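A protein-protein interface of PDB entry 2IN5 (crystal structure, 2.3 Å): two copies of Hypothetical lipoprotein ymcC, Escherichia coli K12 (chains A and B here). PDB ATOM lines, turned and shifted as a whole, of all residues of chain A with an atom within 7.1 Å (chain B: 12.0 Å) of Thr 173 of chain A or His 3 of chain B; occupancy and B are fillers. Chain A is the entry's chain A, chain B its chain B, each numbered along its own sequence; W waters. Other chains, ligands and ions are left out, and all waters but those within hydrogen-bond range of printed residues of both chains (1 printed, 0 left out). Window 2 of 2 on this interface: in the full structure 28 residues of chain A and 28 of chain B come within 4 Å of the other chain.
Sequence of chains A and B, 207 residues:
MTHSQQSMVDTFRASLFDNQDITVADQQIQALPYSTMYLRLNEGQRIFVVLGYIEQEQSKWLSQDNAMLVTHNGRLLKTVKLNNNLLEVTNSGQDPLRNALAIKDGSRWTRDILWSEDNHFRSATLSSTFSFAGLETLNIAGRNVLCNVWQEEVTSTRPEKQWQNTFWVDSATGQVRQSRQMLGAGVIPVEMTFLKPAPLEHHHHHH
OG of Ser 59 of chain A is in hydrogen-bond range of OE1 of Gln 5 of chain B (2.5 Å). The side-chain amide oxygen of Asn 73 of chain A lies within hydrogen-bond range of a ring nitrogen (NE2) of His 3 of chain B.
The side-chain amide nitrogen (ND2) of Asn 73 of chain A lies within hydrogen-bond range of the backbone carbonyl oxygen (O) of Gly 174 of chain A, 3.2 Å away. The side-chain amide oxygen (OD1) of Asn 73 of chain A lies within hydrogen-bond range of the backbone NH (N) of Val 176 of chain A, 3.2 Å away. OD1 of Asp 170 of chain A sits at hydrogen-bond distance from N of Thr 173 of chain A, at 3.0 Å. N of Asp 170 of chain A is in hydrogen-bond range of O of Gln 175 of chain A (2.9 Å). The backbone NH (N) of Gln 175 of chain A lies within hydrogen-bond range of the side-chain hydroxyl (OG1) of Thr 173 of chain A. The side-chain amide oxygen of Gln 175 of chain A sits at hydrogen-bond distance from the backbone NH of Ala 198 of chain A, 3.2 Å away.
Among the printed residues, pairs that only touch across the chains: Thr 173 of chain A with His 3 of chain B (3.6 Å), Gln 175 of chain A with His 3 of chain B (3.3 Å), Lys 196 of chain A with Gln 6 of chain B (3.7 Å), Ala 198 of chain A with His 3 of chain B (3.9 Å) and Ala 198 of chain A with Ser 4 of chain B (3.2 Å).
Of the printed residues of chain B, Ser 59 of chain A touches Gln 5 (2.5 Å). Asn 73 of chain A touches one residue of chain B. Gly 74 of chain A touches none of the printed residues of chain B. No residue of chain B comes within 4 Å of Ala 100 of chain A. No residue of chain B comes within 4 Å of Ser 171 of chain A. Thr 173 of chain A touches one residue of chain B. No residue of chain B comes within 4 Å of Gly 174 of chain A. Gln 175 of chain A touches just one residue of chain B: His 3. No residue of chain B comes within 4 Å of Val 176 of chain A. Of the printed residues of chain B, Lys 196 of chain A touches Gln 6. Pro 197 of chain A touches none of the printed residues of chain B. No residue of chain B comes within 4 Å of Pro 199 of chain A. His 3 of chain B touches just these residues of chain A: Asn 73, Thr 173, Gln 175 and Ala 198. Printed residues of chain A within 4 Å of Gln 6 of chain B: Lys 196 (3.7 Å). The nearest printed residue of chain B that does not touch Lys 196 of chain A is Gln 5 of chain B (5.9 Å).
Of the 21 printed residues of chain A, 6 touch a printed residue of chain B. Hydrophobic or aromatic side chains of chain A that line the printed part of chain B: Ala 198. Of the 6 printed residues of chain B, 4 touch a printed residue of chain A. Printed residues of chain B that touch a printed residue of chain A: His 3, Ser 4, Gln 5 and Gln 6.
No position is printed for both chains. Of the 7 pairs that touch across the chains among the printed residues, none has its exchanged pair printed and touching as well.
Water W1 bridges the side-chain amide nitrogen (NE2) of Gln 5 of chain B and the side-chain amide nitrogen (NE2) of Gln 175 of chain A.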
ATOM      1  N   SER A  59      10.359   5.573 -16.710  1.00  0.00           N
ATOM      2  CA  SER A  59       9.261   5.765 -15.768  1.00  0.00           C
ATOM      3  C   SER A  59       9.316   7.153 -15.150  1.00  0.00           C
ATOM      4  O   SER A  59      10.302   7.503 -14.510  1.00  0.00           O
ATOM      5  CB  SER A  59       9.334   4.722 -14.649  1.00  0.00           C
ATOM      6  OG  SER A  59       9.154   3.408 -15.145  1.00  0.00           O
ATOM      7  N   HIS A  72      14.619   3.873 -14.416  1.00  0.00           N
ATOM      8  CA  HIS A  72      14.437   2.670 -15.187  1.00  0.00           C
ATOM      9  C   HIS A  72      14.868   1.541 -14.270  1.00  0.00           C
ATOM     10  O   HIS A  72      16.042   1.415 -13.913  1.00  0.00           O
ATOM     11  CB  HIS A  72      15.231   2.616 -16.483  1.00  0.00           C
ATOM     12  CG  HIS A  72      14.976   1.351 -17.240  1.00  0.00           C
ATOM     13  ND1 HIS A  72      15.611   0.166 -16.932  1.00  0.00           N
ATOM     14  CD2 HIS A  72      14.034   1.042 -18.160  1.00  0.00           C
ATOM     15  CE1 HIS A  72      15.067  -0.815 -17.625  1.00  0.00           C
ATOM     16  NE2 HIS A  72      14.106  -0.311 -18.375  1.00  0.00           N
ATOM     17  N   ASN A  73      13.890   0.739 -13.871  1.00  0.00           N
ATOM     18  CA  ASN A  73      14.105  -0.375 -12.961  1.00  0.00           C
ATOM     19  C   ASN A  73      14.963  -0.022 -11.751  1.00  0.00           C
ATOM     20  O   ASN A  73      16.021  -0.626 -11.514  1.00  0.00           O
ATOM     21  CB  ASN A  73      14.705  -1.580 -13.687  1.00  0.00           C
ATOM     22  CG  ASN A  73      14.285  -2.888 -13.044  1.00  0.00           C
ATOM     23  OD1 ASN A  73      13.170  -2.994 -12.541  1.00  0.00           O
ATOM     24  ND2 ASN A  73      15.162  -3.889 -13.067  1.00  0.00           N
ATOM     25  N   GLY A  74      14.489   0.970 -10.995  1.00  0.00           N
ATOM     26  CA  GLY A  74      15.168   1.399  -9.783  1.00  0.00           C
ATOM     27  C   GLY A  74      16.351   2.329  -9.952  1.00  0.00           C
ATOM     28  O   GLY A  74      16.799   2.939  -8.975  1.00  0.00           O
ATOM     29  N   LEU A  97      20.846  -3.377 -14.673  1.00  0.00           N
ATOM     30  CA  LEU A  97      19.495  -3.385 -14.155  1.00  0.00           C
ATOM     31  C   LEU A  97      18.477  -3.454 -15.278  1.00  0.00           C
ATOM     32  O   LEU A  97      17.285  -3.632 -15.027  1.00  0.00           O
ATOM     33  CB  LEU A  97      19.244  -2.142 -13.312  1.00  0.00           C
ATOM     34  CG  LEU A  97      20.041  -2.104 -12.010  1.00  0.00           C
ATOM     35  CD1 LEU A  97      19.873  -0.750 -11.340  1.00  0.00           C
ATOM     36  CD2 LEU A  97      19.559  -3.223 -11.100  1.00  0.00           C
ATOM     37  N   ALA A 100      17.707  -7.212 -14.822  1.00  0.00           N
ATOM     38  CA  ALA A 100      18.042  -7.554 -13.440  1.00  0.00           C
ATOM     39  C   ALA A 100      18.153  -9.038 -13.123  1.00  0.00           C
ATOM     40  O   ALA A 100      18.938  -9.424 -12.267  1.00  0.00           O
ATOM     41  CB  ALA A 100      17.042  -6.890 -12.489  1.00  0.00           C
ATOM     42  N   LEU A 101      17.371  -9.876 -13.788  1.00  0.00           N
ATOM     43  CA  LEU A 101      17.462 -11.302 -13.510  1.00  0.00           C
ATOM     44  C   LEU A 101      18.702 -11.935 -14.145  1.00  0.00           C
ATOM     45  O   LEU A 101      19.232 -12.912 -13.619  1.00  0.00           O
ATOM     46  CB  LEU A 101      16.200 -12.024 -13.983  1.00  0.00           C
ATOM     47  CG  LEU A 101      14.956 -11.815 -13.122  1.00  0.00           C
ATOM     48  CD1 LEU A 101      13.825 -12.635 -13.705  1.00  0.00           C
ATOM     49  CD2 LEU A 101      15.220 -12.228 -11.671  1.00  0.00           C
ATOM     50  N   VAL A 169      16.228  -6.846  -5.822  1.00  0.00           N
ATOM     51  CA  VAL A 169      15.506  -7.359  -6.986  1.00  0.00           C
ATOM     52  C   VAL A 169      14.580  -8.543  -6.724  1.00  0.00           C
ATOM     53  O   VAL A 169      14.953  -9.492  -6.044  1.00  0.00           O
ATOM     54  CB  VAL A 169      16.505  -7.798  -8.087  1.00  0.00           C
ATOM     55  CG1 VAL A 169      15.757  -8.211  -9.340  1.00  0.00           C
ATOM     56  CG2 VAL A 169      17.487  -6.679  -8.371  1.00  0.00           C
ATOM     57  N   ASP A 170      13.381  -8.485  -7.287  1.00  0.00           N
ATOM     58  CA  ASP A 170      12.428  -9.575  -7.163  1.00  0.00           C
ATOM     59  C   ASP A 170      13.019 -10.747  -7.959  1.00  0.00           C
ATOM     60  O   ASP A 170      13.079 -10.693  -9.184  1.00  0.00           O
ATOM     61  CB  ASP A 170      11.086  -9.171  -7.760  1.00  0.00           C
ATOM     62  CG  ASP A 170      10.033 -10.252  -7.606  1.00  0.00           C
ATOM     63  OD1 ASP A 170      10.213 -11.361  -8.155  1.00  0.00           O
ATOM     64  OD2 ASP A 170       9.029  -9.986  -6.925  1.00  0.00           O
ATOM     65  N   SER A 171      13.436 -11.800  -7.261  1.00  0.00           N
ATOM     66  CA  SER A 171      14.070 -12.965  -7.881  1.00  0.00           C
ATOM     67  C   SER A 171      13.270 -13.725  -8.943  1.00  0.00           C
ATOM     68  O   SER A 171      13.795 -14.650  -9.555  1.00  0.00           O
ATOM     69  CB  SER A 171      14.496 -13.952  -6.788  1.00  0.00           C
ATOM     70  OG  SER A 171      13.367 -14.476  -6.111  1.00  0.00           O
ATOM     71  N   ALA A 172      12.015 -13.327  -9.149  1.00  0.00           N
ATOM     72  CA  ALA A 172      11.116 -13.967 -10.106  1.00  0.00           C
ATOM     73  C   ALA A 172      10.748 -13.084 -11.302  1.00  0.00           C
ATOM     74  O   ALA A 172      10.561 -13.572 -12.420  1.00  0.00           O
ATOM     75  CB  ALA A 172       9.844 -14.408  -9.392  1.00  0.00           C
ATOM     76  N   THR A 173      10.636 -11.781 -11.075  1.00  0.00           N
ATOM     77  CA  THR A 173      10.276 -10.870 -12.160  1.00  0.00           C
ATOM     78  C   THR A 173      11.452 -10.040 -12.639  1.00  0.00           C
ATOM     79  O   THR A 173      11.529  -9.692 -13.806  1.00  0.00           O
ATOM     80  CB  THR A 173       9.170  -9.900 -11.722  1.00  0.00           C
ATOM     81  OG1 THR A 173       9.669  -9.062 -10.672  1.00  0.00           O
ATOM     82  CG2 THR A 173       7.959 -10.658 -11.241  1.00  0.00           C
ATOM     83  N   GLY A 174      12.362  -9.726 -11.728  1.00  0.00           N
ATOM     84  CA  GLY A 174      13.506  -8.915 -12.087  1.00  0.00           C
ATOM     85  C   GLY A 174      13.258  -7.468 -11.709  1.00  0.00           C
ATOM     86  O   GLY A 174      14.144  -6.627 -11.825  1.00  0.00           O
ATOM     87  N   GLN A 175      12.042  -7.172 -11.261  1.00  0.00           N
ATOM     88  CA  GLN A 175      11.688  -5.816 -10.852  1.00  0.00           C
ATOM     89  C   GLN A 175      12.389  -5.414  -9.566  1.00  0.00           C
ATOM     90  O   GLN A 175      12.372  -6.155  -8.598  1.00  0.00           O
ATOM     91  CB  GLN A 175      10.173  -5.684 -10.637  1.00  0.00           C
ATOM     92  CG  GLN A 175       9.794  -4.366  -9.934  1.00  0.00           C
ATOM     93  CD  GLN A 175       8.336  -4.296  -9.509  1.00  0.00           C
ATOM     94  OE1 GLN A 175       7.804  -5.230  -8.914  1.00  0.00           O
ATOM     95  NE2 GLN A 175       7.693  -3.174  -9.793  1.00  0.00           N
ATOM     96  N   VAL A 176      13.004  -4.235  -9.566  1.00  0.00           N
ATOM     97  CA  VAL A 176      13.677  -3.717  -8.381  1.00  0.00           C
ATOM     98  C   VAL A 176      12.555  -3.204  -7.468  1.00  0.00           C
ATOM     99  O   VAL A 176      11.692  -2.448  -7.912  1.00  0.00           O
ATOM    100  CB  VAL A 176      14.645  -2.566  -8.772  1.00  0.00           C
ATOM    101  CG1 VAL A 176      15.154  -1.831  -7.530  1.00  0.00           C
ATOM    102  CG2 VAL A 176      15.817  -3.140  -9.562  1.00  0.00           C
ATOM    103  N   ARG A 177      12.547  -3.639  -6.211  1.00  0.00           N
ATOM    104  CA  ARG A 177      11.507  -3.221  -5.279  1.00  0.00           C
ATOM    105  C   ARG A 177      12.012  -2.193  -4.286  1.00  0.00           C
ATOM    106  O   ARG A 177      11.234  -1.547  -3.585  1.00  0.00           O
ATOM    107  CB  ARG A 177      10.939  -4.426  -4.517  1.00  0.00           C
ATOM    108  CG  ARG A 177      10.158  -5.410  -5.367  1.00  0.00           C
ATOM    109  CD  ARG A 177       9.028  -4.742  -6.138  1.00  0.00           C
ATOM    110  NE  ARG A 177       7.998  -4.138  -5.290  1.00  0.00           N
ATOM    111  CZ  ARG A 177       7.105  -4.817  -4.575  1.00  0.00           C
ATOM    112  NH1 ARG A 177       7.099  -6.146  -4.592  1.00  0.00           N
ATOM    113  NH2 ARG A 177       6.211  -4.160  -3.851  1.00  0.00           N
ATOM    114  N   LYS A 196       3.886  -1.019  -5.428  1.00  0.00           N
ATOM    115  CA  LYS A 196       3.062  -1.921  -6.211  1.00  0.00           C
ATOM    116  C   LYS A 196       3.900  -3.008  -6.855  1.00  0.00           C
ATOM    117  O   LYS A 196       4.779  -2.736  -7.671  1.00  0.00           O
ATOM    118  CB  LYS A 196       2.286  -1.142  -7.257  1.00  0.00           C
ATOM    119  CG  LYS A 196       1.428  -1.999  -8.126  1.00  0.00           C
ATOM    120  CD  LYS A 196       0.524  -1.135  -8.957  1.00  0.00           C
ATOM    121  CE  LYS A 196      -0.174  -1.990  -9.953  1.00  0.00           C
ATOM    122  NZ  LYS A 196      -0.689  -3.170  -9.221  1.00  0.00           N
ATOM    123  N   PRO A 197       3.642  -4.268  -6.478  1.00  0.00           N
ATOM    124  CA  PRO A 197       4.347  -5.447  -6.983  1.00  0.00           C
ATOM    125  C   PRO A 197       3.871  -5.858  -8.365  1.00  0.00           C
ATOM    126  O   PRO A 197       2.681  -5.812  -8.652  1.00  0.00           O
ATOM    127  CB  PRO A 197       4.033  -6.498  -5.932  1.00  0.00           C
ATOM    128  CG  PRO A 197       2.623  -6.163  -5.571  1.00  0.00           C
ATOM    129  CD  PRO A 197       2.671  -4.653  -5.435  1.00  0.00           C
ATOM    130  N   ALA A 198       4.807  -6.257  -9.220  1.00  0.00           N
ATOM    131  CA  ALA A 198       4.471  -6.686 -10.575  1.00  0.00           C
ATOM    132  C   ALA A 198       4.353  -8.214 -10.642  1.00  0.00           C
ATOM    133  O   ALA A 198       5.180  -8.940 -10.083  1.00  0.00           O
ATOM    134  CB  ALA A 198       5.530  -6.187 -11.562  1.00  0.00           C
ATOM    135  N   PRO A 199       3.310  -8.719 -11.319  1.00  0.00           N
ATOM    136  CA  PRO A 199       3.071 -10.158 -11.466  1.00  0.00           C
ATOM    137  C   PRO A 199       3.950 -10.768 -12.544  1.00  0.00           C
ATOM    138  O   PRO A 199       4.747 -10.076 -13.183  1.00  0.00           O
ATOM    139  CB  PRO A 199       1.598 -10.221 -11.848  1.00  0.00           C
ATOM    140  CG  PRO A 199       1.456  -9.012 -12.718  1.00  0.00           C
ATOM    141  CD  PRO A 199       2.204  -7.946 -11.919  1.00  0.00           C
ATOM    142  N   LEU A 200       3.800 -12.073 -12.739  1.00  0.00           N
ATOM    143  CA  LEU A 200       4.561 -12.768 -13.761  1.00  0.00           C
ATOM    144  C   LEU A 200       3.710 -12.850 -15.032  1.00  0.00           C
ATOM    145  O   LEU A 200       4.242 -12.513 -16.118  1.00  0.00           O
ATOM    146  CB  LEU A 200       4.964 -14.169 -13.276  1.00  0.00           C
ATOM    147  CG  LEU A 200       5.960 -14.235 -12.108  1.00  0.00           C
ATOM    148  CD1 LEU A 200       5.259 -13.873 -10.806  1.00  0.00           C
ATOM    149  CD2 LEU A 200       6.552 -15.632 -12.016  1.00  0.00           C
ATOM    150  N   HIS B   3       8.353  -8.485 -15.755  1.00  0.00           N
ATOM    151  CA  HIS B   3       8.257  -7.175 -15.041  1.00  0.00           C
ATOM    152  C   HIS B   3       7.574  -6.080 -15.870  1.00  0.00           C
ATOM    153  O   HIS B   3       7.949  -5.814 -17.016  1.00  0.00           O
ATOM    154  CB  HIS B   3       9.658  -6.719 -14.606  1.00  0.00           C
ATOM    155  CG  HIS B   3       9.713  -5.307 -14.111  1.00  0.00           C
ATOM    156  ND1 HIS B   3       8.661  -4.703 -13.455  1.00  0.00           N
ATOM    157  CD2 HIS B   3      10.702  -4.384 -14.164  1.00  0.00           C
ATOM    158  CE1 HIS B   3       8.999  -3.468 -13.127  1.00  0.00           C
ATOM    159  NE2 HIS B   3      10.232  -3.249 -13.545  1.00  0.00           N
ATOM    160  N   SER B   4       6.561  -5.459 -15.269  1.00  0.00           N
ATOM    161  CA  SER B   4       5.797  -4.386 -15.899  1.00  0.00           C
ATOM    162  C   SER B   4       5.232  -3.459 -14.816  1.00  0.00           C
ATOM    163  O   SER B   4       5.091  -3.861 -13.660  1.00  0.00           O
ATOM    164  CB  SER B   4       4.649  -4.967 -16.726  1.00  0.00           C
ATOM    165  OG  SER B   4       3.999  -3.955 -17.473  1.00  0.00           O
ATOM    166  N   GLN B   5       4.913  -2.224 -15.189  1.00  0.00           N
ATOM    167  CA  GLN B   5       4.378  -1.263 -14.235  1.00  0.00           C
ATOM    168  C   GLN B   5       3.038  -0.726 -14.677  1.00  0.00           C
ATOM    169  O   GLN B   5       2.653  -0.869 -15.835  1.00  0.00           O
ATOM    170  CB  GLN B   5       5.341  -0.103 -14.057  1.00  0.00           C
ATOM    171  CG  GLN B   5       6.719  -0.527 -13.630  1.00  0.00           C
ATOM    172  CD  GLN B   5       7.667   0.646 -13.555  1.00  0.00           C
ATOM    173  OE1 GLN B   5       7.729   1.464 -14.469  1.00  0.00           O
ATOM    174  NE2 GLN B   5       8.418   0.731 -12.470  1.00  0.00           N
ATOM    175  N   GLN B   6       2.323  -0.115 -13.741  1.00  0.00           N
ATOM    176  CA  GLN B   6       1.020   0.459 -14.031  1.00  0.00           C
ATOM    177  C   GLN B   6       1.121   1.952 -13.746  1.00  0.00           C
ATOM    178  O   GLN B   6       1.324   2.364 -12.607  1.00  0.00           O
ATOM    179  CB  GLN B   6      -0.046  -0.173 -13.135  1.00  0.00           C
ATOM    180  CG  GLN B   6      -1.475   0.194 -13.498  1.00  0.00           C
ATOM    181  CD  GLN B   6      -1.909  -0.416 -14.816  1.00  0.00           C
ATOM    182  OE1 GLN B   6      -1.204  -1.251 -15.385  1.00  0.00           O
ATOM    183  NE2 GLN B   6      -3.080  -0.017 -15.301  1.00  0.00           N
ATOM    184  N   SER B   7       1.007   2.754 -14.791  1.00  0.00           N
ATOM    185  CA  SER B   7       1.088   4.188 -14.652  1.00  0.00           C
ATOM    186  C   SER B   7      -0.328   4.715 -14.634  1.00  0.00           C
ATOM    187  O   SER B   7      -1.256   4.018 -15.045  1.00  0.00           O
ATOM    188  CB  SER B   7       1.803   4.797 -15.852  1.00  0.00           C
ATOM    189  OG  SER B   7       0.942   4.741 -16.975  1.00  0.00           O
ATOM    190  N   ASP B  10      -2.007   4.505 -17.961  1.00  0.00           N
ATOM    191  CA  ASP B  10      -2.481   3.166 -18.270  1.00  0.00           C
ATOM    192  C   ASP B  10      -3.862   3.015 -17.625  1.00  0.00           C
ATOM    193  O   ASP B  10      -4.787   2.491 -18.238  1.00  0.00           O
ATOM    194  CB  ASP B  10      -1.540   2.099 -17.689  1.00  0.00           C
ATOM    195  CG  ASP B  10      -0.219   2.008 -18.421  1.00  0.00           C
ATOM    196  OD1 ASP B  10       0.795   1.616 -17.767  1.00  0.00           O
ATOM    197  OD2 ASP B  10      -0.186   2.310 -19.646  1.00  0.00           O
HETATM  198  O   HOH W   1       7.316  -0.238 -10.116  1.00  0.00           O
